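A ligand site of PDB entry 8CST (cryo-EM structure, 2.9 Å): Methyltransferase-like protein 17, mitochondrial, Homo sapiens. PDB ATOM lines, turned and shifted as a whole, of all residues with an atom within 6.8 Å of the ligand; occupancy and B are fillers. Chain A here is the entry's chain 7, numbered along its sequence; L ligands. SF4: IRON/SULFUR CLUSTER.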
ATOM      1  N   HIS A 303     -28.094  12.065   1.418  1.00  0.00           N
ATOM      2  CA  HIS A 303     -26.877  11.958   2.208  1.00  0.00           C
ATOM      3  C   HIS A 303     -25.825  12.952   1.737  1.00  0.00           C
ATOM      4  O   HIS A 303     -25.165  13.608   2.554  1.00  0.00           O
ATOM      5  CB  HIS A 303     -26.328  10.535   2.152  1.00  0.00           C
ATOM      6  CG  HIS A 303     -25.047  10.366   2.895  1.00  0.00           C
ATOM      7  ND1 HIS A 303     -23.873   9.979   2.281  1.00  0.00           N
ATOM      8  CD2 HIS A 303     -24.744  10.542   4.206  1.00  0.00           C
ATOM      9  CE1 HIS A 303     -22.913   9.913   3.180  1.00  0.00           C
ATOM     10  NE2 HIS A 303     -23.405  10.258   4.355  1.00  0.00           N
ATOM     11  N   MET A 307     -24.340  15.948   4.011  1.00  0.00           N
ATOM     12  CA  MET A 307     -22.902  16.014   4.265  1.00  0.00           C
ATOM     13  C   MET A 307     -22.286  17.319   3.796  1.00  0.00           C
ATOM     14  O   MET A 307     -21.382  17.848   4.453  1.00  0.00           O
ATOM     15  CB  MET A 307     -22.171  14.832   3.647  1.00  0.00           C
ATOM     16  CG  MET A 307     -22.487  13.474   4.236  1.00  0.00           C
ATOM     17  SD  MET A 307     -22.003  13.510   5.985  1.00  0.00           S
ATOM     18  CE  MET A 307     -20.218  13.609   5.825  1.00  0.00           C
ATOM     19  N   ARG A 310     -23.102  19.555   6.496  1.00  0.00           N
ATOM     20  CA  ARG A 310     -22.320  19.248   7.688  1.00  0.00           C
ATOM     21  C   ARG A 310     -20.925  19.857   7.571  1.00  0.00           C
ATOM     22  O   ARG A 310     -20.424  20.477   8.509  1.00  0.00           O
ATOM     23  CB  ARG A 310     -22.214  17.734   7.883  1.00  0.00           C
ATOM     24  CG  ARG A 310     -21.393  17.332   9.103  1.00  0.00           C
ATOM     25  CD  ARG A 310     -21.374  15.828   9.323  1.00  0.00           C
ATOM     26  NE  ARG A 310     -20.278  15.210   8.587  1.00  0.00           N
ATOM     27  CZ  ARG A 310     -19.210  14.633   9.125  1.00  0.00           C
ATOM     28  NH1 ARG A 310     -19.109  14.422  10.428  1.00  0.00           N
ATOM     29  NH2 ARG A 310     -18.220  14.237   8.338  1.00  0.00           N
ATOM     30  N   VAL A 329     -20.561  17.818  15.607  1.00  0.00           N
ATOM     31  CA  VAL A 329     -21.627  16.919  15.186  1.00  0.00           C
ATOM     32  C   VAL A 329     -22.090  16.128  16.396  1.00  0.00           C
ATOM     33  O   VAL A 329     -21.385  15.242  16.886  1.00  0.00           O
ATOM     34  CB  VAL A 329     -21.174  15.981  14.061  1.00  0.00           C
ATOM     35  CG1 VAL A 329     -22.356  15.278  13.452  1.00  0.00           C
ATOM     36  CG2 VAL A 329     -20.417  16.774  13.004  1.00  0.00           C
ATOM     37  N   ALA A 331     -24.986  14.217  16.512  1.00  0.00           N
ATOM     38  CA  ALA A 331     -25.472  12.943  16.025  1.00  0.00           C
ATOM     39  C   ALA A 331     -25.764  13.092  14.536  1.00  0.00           C
ATOM     40  O   ALA A 331     -26.005  14.204  14.058  1.00  0.00           O
ATOM     41  CB  ALA A 331     -26.738  12.490  16.773  1.00  0.00           C
ATOM     42  N   PRO A 332     -25.767  11.985  13.778  1.00  0.00           N
ATOM     43  CA  PRO A 332     -25.469  10.611  14.156  1.00  0.00           C
ATOM     44  C   PRO A 332     -23.992  10.255  14.024  1.00  0.00           C
ATOM     45  O   PRO A 332     -23.629   9.098  14.209  1.00  0.00           O
ATOM     46  CB  PRO A 332     -26.295   9.810  13.170  1.00  0.00           C
ATOM     47  CG  PRO A 332     -26.260  10.630  11.930  1.00  0.00           C
ATOM     48  CD  PRO A 332     -26.151  12.073  12.364  1.00  0.00           C
ATOM     49  N   CYS A 333     -23.163  11.239  13.700  1.00  0.00           N
ATOM     50  CA  CYS A 333     -21.755  10.958  13.493  1.00  0.00           C
ATOM     51  C   CYS A 333     -20.992  11.046  14.814  1.00  0.00           C
ATOM     52  O   CYS A 333     -21.161  12.014  15.558  1.00  0.00           O
ATOM     53  CB  CYS A 333     -21.163  11.928  12.491  1.00  0.00           C
ATOM     54  SG  CYS A 333     -22.206  12.183  11.041  1.00  0.00           S
ATOM     55  N   PRO A 334     -20.145  10.071  15.155  1.00  0.00           N
ATOM     56  CA  PRO A 334     -19.368  10.171  16.400  1.00  0.00           C
ATOM     57  C   PRO A 334     -18.029  10.876  16.208  1.00  0.00           C
ATOM     58  O   PRO A 334     -17.171  10.815  17.092  1.00  0.00           O
ATOM     59  CB  PRO A 334     -19.163   8.713  16.794  1.00  0.00           C
ATOM     60  CG  PRO A 334     -19.079   8.005  15.490  1.00  0.00           C
ATOM     61  CD  PRO A 334     -19.923   8.766  14.505  1.00  0.00           C
ATOM     62  N   HIS A 335     -17.845  11.539  15.069  1.00  0.00           N
ATOM     63  CA  HIS A 335     -16.603  12.246  14.792  1.00  0.00           C
ATOM     64  C   HIS A 335     -16.930  13.446  13.907  1.00  0.00           C
ATOM     65  O   HIS A 335     -18.087  13.734  13.619  1.00  0.00           O
ATOM     66  CB  HIS A 335     -15.575  11.349  14.104  1.00  0.00           C
ATOM     67  CG  HIS A 335     -16.066  10.755  12.824  1.00  0.00           C
ATOM     68  ND1 HIS A 335     -16.022  11.430  11.623  1.00  0.00           N
ATOM     69  CD2 HIS A 335     -16.577   9.530  12.546  1.00  0.00           C
ATOM     70  CE1 HIS A 335     -16.513  10.665  10.671  1.00  0.00           C
ATOM     71  NE2 HIS A 335     -16.846   9.498  11.194  1.00  0.00           N
ATOM     72  N   LEU A 337     -14.572  14.048  11.113  1.00  0.00           N
ATOM     73  CA  LEU A 337     -13.815  13.806   9.891  1.00  0.00           C
ATOM     74  C   LEU A 337     -14.775  13.497   8.752  1.00  0.00           C
ATOM     75  O   LEU A 337     -15.954  13.240   8.975  1.00  0.00           O
ATOM     76  CB  LEU A 337     -12.845  12.653  10.124  1.00  0.00           C
ATOM     77  CG  LEU A 337     -11.581  12.994  10.904  1.00  0.00           C
ATOM     78  CD1 LEU A 337     -11.903  13.258  12.367  1.00  0.00           C
ATOM     79  CD2 LEU A 337     -10.564  11.865  10.780  1.00  0.00           C
ATOM     80  N   PRO A 338     -14.294  13.535   7.507  1.00  0.00           N
ATOM     81  CA  PRO A 338     -15.157  13.193   6.374  1.00  0.00           C
ATOM     82  C   PRO A 338     -15.729  11.788   6.518  1.00  0.00           C
ATOM     83  O   PRO A 338     -15.116  10.900   7.105  1.00  0.00           O
ATOM     84  CB  PRO A 338     -14.231  13.295   5.163  1.00  0.00           C
ATOM     85  CG  PRO A 338     -12.849  13.352   5.722  1.00  0.00           C
ATOM     86  CD  PRO A 338     -12.983  14.025   7.042  1.00  0.00           C
ATOM     87  N   CYS A 339     -16.931  11.624   5.996  1.00  0.00           N
ATOM     88  CA  CYS A 339     -17.609  10.342   6.103  1.00  0.00           C
ATOM     89  C   CYS A 339     -16.829   9.245   5.378  1.00  0.00           C
ATOM     90  O   CYS A 339     -16.333   9.479   4.261  1.00  0.00           O
ATOM     91  CB  CYS A 339     -19.011  10.422   5.502  1.00  0.00           C
ATOM     92  SG  CYS A 339     -19.985   8.965   5.809  1.00  0.00           S
ATOM     93  N   PRO A 340     -16.703   8.061   5.956  1.00  0.00           N
ATOM     94  CA  PRO A 340     -16.190   6.920   5.180  1.00  0.00           C
ATOM     95  C   PRO A 340     -17.206   6.333   4.208  1.00  0.00           C
ATOM     96  O   PRO A 340     -16.851   5.404   3.471  1.00  0.00           O
ATOM     97  CB  PRO A 340     -15.814   5.910   6.257  1.00  0.00           C
ATOM     98  CG  PRO A 340     -16.722   6.231   7.381  1.00  0.00           C
ATOM     99  CD  PRO A 340     -16.907   7.698   7.375  1.00  0.00           C
ATOM    100  N   GLN A 341     -18.444   6.821   4.191  1.00  0.00           N
ATOM    101  CA  GLN A 341     -19.507   6.213   3.378  1.00  0.00           C
ATOM    102  C   GLN A 341     -19.937   7.113   2.229  1.00  0.00           C
ATOM    103  O   GLN A 341     -20.774   6.707   1.423  1.00  0.00           O
ATOM    104  CB  GLN A 341     -20.709   5.878   4.253  1.00  0.00           C
ATOM    105  CG  GLN A 341     -20.474   4.746   5.226  1.00  0.00           C
ATOM    106  CD  GLN A 341     -20.848   3.407   4.673  1.00  0.00           C
ATOM    107  OE1 GLN A 341     -19.996   2.646   4.211  1.00  0.00           O
ATOM    108  NE2 GLN A 341     -22.131   3.096   4.714  1.00  0.00           N
ATOM    109  N   LEU A 342     -19.381   8.322   2.118  1.00  0.00           N
ATOM    110  CA  LEU A 342     -19.757   9.215   1.026  1.00  0.00           C
ATOM    111  C   LEU A 342     -19.182   8.785  -0.313  1.00  0.00           C
ATOM    112  O   LEU A 342     -19.720   9.185  -1.352  1.00  0.00           O
ATOM    113  CB  LEU A 342     -19.293  10.643   1.326  1.00  0.00           C
ATOM    114  CG  LEU A 342     -19.662  11.722   0.290  1.00  0.00           C
ATOM    115  CD1 LEU A 342     -21.163  11.779   0.052  1.00  0.00           C
ATOM    116  CD2 LEU A 342     -19.133  13.080   0.711  1.00  0.00           C
ATOM    117  N   ALA A 346     -24.188   5.447   0.780  1.00  0.00           N
ATOM    118  CA  ALA A 346     -24.891   6.464   1.547  1.00  0.00           C
ATOM    119  C   ALA A 346     -24.938   6.039   3.021  1.00  0.00           C
ATOM    120  O   ALA A 346     -24.434   4.980   3.398  1.00  0.00           O
ATOM    121  CB  ALA A 346     -26.298   6.695   1.004  1.00  0.00           C
ATOM    122  N   CYS A 347     -25.540   6.879   3.850  1.00  0.00           N
ATOM    123  CA  CYS A 347     -25.772   6.578   5.248  1.00  0.00           C
ATOM    124  C   CYS A 347     -27.160   7.060   5.626  1.00  0.00           C
ATOM    125  O   CYS A 347     -27.429   8.267   5.597  1.00  0.00           O
ATOM    126  CB  CYS A 347     -24.725   7.241   6.152  1.00  0.00           C
ATOM    127  SG  CYS A 347     -25.118   7.202   7.913  1.00  0.00           S
ATOM    128  N   SER A 348     -28.043   6.129   5.971  1.00  0.00           N
ATOM    129  CA  SER A 348     -29.432   6.428   6.253  1.00  0.00           C
ATOM    130  C   SER A 348     -29.872   5.739   7.540  1.00  0.00           C
ATOM    131  O   SER A 348     -29.154   4.929   8.114  1.00  0.00           O
ATOM    132  CB  SER A 348     -30.343   6.009   5.087  1.00  0.00           C
ATOM    133  OG  SER A 348     -30.074   4.676   4.706  1.00  0.00           O
ATOM    134  N   PHE A 349     -31.086   6.094   7.967  1.00  0.00           N
ATOM    135  CA  PHE A 349     -31.706   5.541   9.160  1.00  0.00           C
ATOM    136  C   PHE A 349     -33.182   5.311   8.852  1.00  0.00           C
ATOM    137  O   PHE A 349     -33.710   5.817   7.856  1.00  0.00           O
ATOM    138  CB  PHE A 349     -31.551   6.473  10.364  1.00  0.00           C
ATOM    139  CG  PHE A 349     -30.122   6.667  10.780  1.00  0.00           C
ATOM    140  CD1 PHE A 349     -29.481   5.717  11.532  1.00  0.00           C
ATOM    141  CD2 PHE A 349     -29.427   7.799  10.396  1.00  0.00           C
ATOM    142  CE1 PHE A 349     -28.170   5.892  11.920  1.00  0.00           C
ATOM    143  CE2 PHE A 349     -28.119   7.980  10.776  1.00  0.00           C
ATOM    144  CZ  PHE A 349     -27.493   7.024  11.543  1.00  0.00           C
ATOM    145  N   MET A 371     -30.159  12.063   8.495  1.00  0.00           N
ATOM    146  CA  MET A 371     -30.258  13.154   9.462  1.00  0.00           C
ATOM    147  C   MET A 371     -28.866  13.634   9.830  1.00  0.00           C
ATOM    148  O   MET A 371     -27.872  12.937   9.625  1.00  0.00           O
ATOM    149  CB  MET A 371     -30.994  12.725  10.729  1.00  0.00           C
ATOM    150  CG  MET A 371     -30.283  11.647  11.540  1.00  0.00           C
ATOM    151  SD  MET A 371     -31.180  11.196  13.032  1.00  0.00           S
ATOM    152  CE  MET A 371     -30.918  12.662  14.008  1.00  0.00           C
ATOM    153  N   ARG A 387     -21.794   4.342  15.943  1.00  0.00           N
ATOM    154  CA  ARG A 387     -23.171   4.454  15.519  1.00  0.00           C
ATOM    155  C   ARG A 387     -23.475   3.336  14.535  1.00  0.00           C
ATOM    156  O   ARG A 387     -22.691   3.091  13.609  1.00  0.00           O
ATOM    157  CB  ARG A 387     -23.435   5.817  14.893  1.00  0.00           C
ATOM    158  CG  ARG A 387     -24.802   5.990  14.236  1.00  0.00           C
ATOM    159  CD  ARG A 387     -25.890   6.317  15.253  1.00  0.00           C
ATOM    160  NE  ARG A 387     -25.549   7.453  16.105  1.00  0.00           N
ATOM    161  CZ  ARG A 387     -26.335   7.937  17.053  1.00  0.00           C
ATOM    162  NH1 ARG A 387     -27.534   7.444  17.277  1.00  0.00           N
ATOM    163  NH2 ARG A 387     -25.903   8.959  17.794  1.00  0.00           N
ATOM    164  N   THR A 389     -25.365   2.130  11.471  1.00  0.00           N
ATOM    165  CA  THR A 389     -25.949   2.816  10.335  1.00  0.00           C
ATOM    166  C   THR A 389     -26.647   1.862   9.366  1.00  0.00           C
ATOM    167  O   THR A 389     -26.867   2.220   8.211  1.00  0.00           O
ATOM    168  CB  THR A 389     -24.871   3.589   9.592  1.00  0.00           C
ATOM    169  OG1 THR A 389     -23.946   2.668   9.002  1.00  0.00           O
ATOM    170  CG2 THR A 389     -24.123   4.479  10.558  1.00  0.00           C
ATOM    171  N   LEU A 403     -20.548  -0.440  11.986  1.00  0.00           N
ATOM    172  CA  LEU A 403     -20.319   0.673  12.885  1.00  0.00           C
ATOM    173  C   LEU A 403     -19.569   1.782  12.170  1.00  0.00           C
ATOM    174  O   LEU A 403     -18.710   1.513  11.333  1.00  0.00           O
ATOM    175  CB  LEU A 403     -19.521   0.227  14.105  1.00  0.00           C
ATOM    176  CG  LEU A 403     -20.370  -0.191  15.299  1.00  0.00           C
ATOM    177  CD1 LEU A 403     -21.360  -1.257  14.901  1.00  0.00           C
ATOM    178  CD2 LEU A 403     -19.472  -0.677  16.424  1.00  0.00           C
ATOM    179  N   CYS A 404     -19.914   3.021  12.502  1.00  0.00           N
ATOM    180  CA  CYS A 404     -19.107   4.180  12.155  1.00  0.00           C
ATOM    181  C   CYS A 404     -18.336   4.580  13.408  1.00  0.00           C
ATOM    182  O   CYS A 404     -18.901   5.177  14.332  1.00  0.00           O
ATOM    183  CB  CYS A 404     -19.976   5.327  11.655  1.00  0.00           C
ATOM    184  SG  CYS A 404     -19.073   6.751  11.052  1.00  0.00           S
ATOM    185  N   CYS A 405     -17.048   4.247  13.453  1.00  0.00           N
ATOM    186  CA  CYS A 405     -16.293   4.382  14.694  1.00  0.00           C
ATOM    187  C   CYS A 405     -15.764   5.798  14.855  1.00  0.00           C
ATOM    188  O   CYS A 405     -15.648   6.548  13.891  1.00  0.00           O
ATOM    189  CB  CYS A 405     -15.149   3.387  14.716  1.00  0.00           C
ATOM    190  SG  CYS A 405     -15.653   1.704  14.314  1.00  0.00           S
ATOM    191  N   HIS A 409     -13.825   5.582  10.599  1.00  0.00           N
ATOM    192  CA  HIS A 409     -13.794   4.430   9.713  1.00  0.00           C
ATOM    193  C   HIS A 409     -15.054   3.590   9.900  1.00  0.00           C
ATOM    194  O   HIS A 409     -15.665   3.592  10.969  1.00  0.00           O
ATOM    195  CB  HIS A 409     -12.562   3.576   9.980  1.00  0.00           C
ATOM    196  CG  HIS A 409     -11.350   4.021   9.230  1.00  0.00           C
ATOM    197  ND1 HIS A 409     -11.382   4.371   7.896  1.00  0.00           N
ATOM    198  CD2 HIS A 409     -10.060   4.175   9.621  1.00  0.00           C
ATOM    199  CE1 HIS A 409     -10.170   4.719   7.496  1.00  0.00           C
ATOM    200  NE2 HIS A 409      -9.352   4.613   8.532  1.00  0.00           N
ATOM    201  N   MET A 410     -15.423   2.861   8.843  1.00  0.00           N
ATOM    202  CA  MET A 410     -16.491   1.884   8.960  1.00  0.00           C
ATOM    203  C   MET A 410     -15.909   0.542   9.346  1.00  0.00           C
ATOM    204  O   MET A 410     -14.938   0.070   8.745  1.00  0.00           O
ATOM    205  CB  MET A 410     -17.262   1.726   7.652  1.00  0.00           C
ATOM    206  CG  MET A 410     -18.028   2.946   7.216  1.00  0.00           C
ATOM    207  SD  MET A 410     -19.278   3.494   8.403  1.00  0.00           S
ATOM    208  CE  MET A 410     -20.490   2.193   8.291  1.00  0.00           C
HETATM  209 FE1  SF4 L   1     -20.827   7.890  10.168  1.00  0.00          FE
HETATM  210 FE2  SF4 L   1     -23.239   8.039   8.847  1.00  0.00          FE
HETATM  211 FE3  SF4 L   1     -22.130  10.233   9.940  1.00  0.00          FE
HETATM  212 FE4  SF4 L   1     -21.023   9.079   7.798  1.00  0.00          FE
HETATM  213  S1  SF4 L   1     -23.100  10.013   7.861  1.00  0.00           S
HETATM  214  S2  SF4 L   1     -19.884   9.832   9.640  1.00  0.00           S
HETATM  215  S3  SF4 L   1     -21.387   6.870   8.162  1.00  0.00           S
HETATM  216  S4  SF4 L   1     -22.852   8.454  11.086  1.00  0.00           S
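S4 of the ligand sits close to O of Pro 332 (3.3 Å). Residues that only touch the ligand: Gln 341 (3.7 Å) and Met 410 (3.99 Å). Hydrophobic or aromatic side chains within 4 Å of the ligand: His 335 and Met 410. Of the 27 residues printed, 9 come within 4 Å of the ligand.
A ring nitrogen (NE2) of His 335 lies close to the side-chain sulfur (SG) of Cys 404, 3.5 Å away. The side-chain sulfur (SG) of Cys 339 lies close to the backbone NH (N) of Gln 341, at 3.1 Å. ND1 of His 335 is in hydrogen-bond range of N of Leu 337 (3.0 Å). The side-chain sulfur of Cys 339 lies close to the backbone NH of Leu 342. NE2 of Gln 341 lies within hydrogen-bond range of O of Ala 346 (3.3 Å). The backbone carbonyl oxygen (O) of Arg 387 is in hydrogen-bond range of the backbone NH (N) of Cys 404 (3.0 Å). The backbone carbonyl oxygen (O) of His 335 lies within hydrogen-bond range of the guanidinium group (NH1) of Arg 310, 3.4 Å away. NE of Arg 387 lies within hydrogen-bond range of O of Pro 332.
An iron atom (FE1) of the ligand is bound by the side-chain sulfur (SG) of Cys 404, at 2.3 Å. NE2 of His 303 lies close to S1 of the ligand (3.5 Å). A ring nitrogen (NE2) of His 335 sits close to a sulfur (S2) of the ligand (3.4 Å). An iron atom (FE2) of the ligand is bound by the side-chain sulfur of Cys 347, 2.3 Å away. The side-chain sulfur of Cys 339 is bound to an iron atom (FE4) of the ligand, 2.2 Å away. The side-chain sulfur of Cys 333 is bound to an iron atom (FE3) of the ligand, 2.2 Å away.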
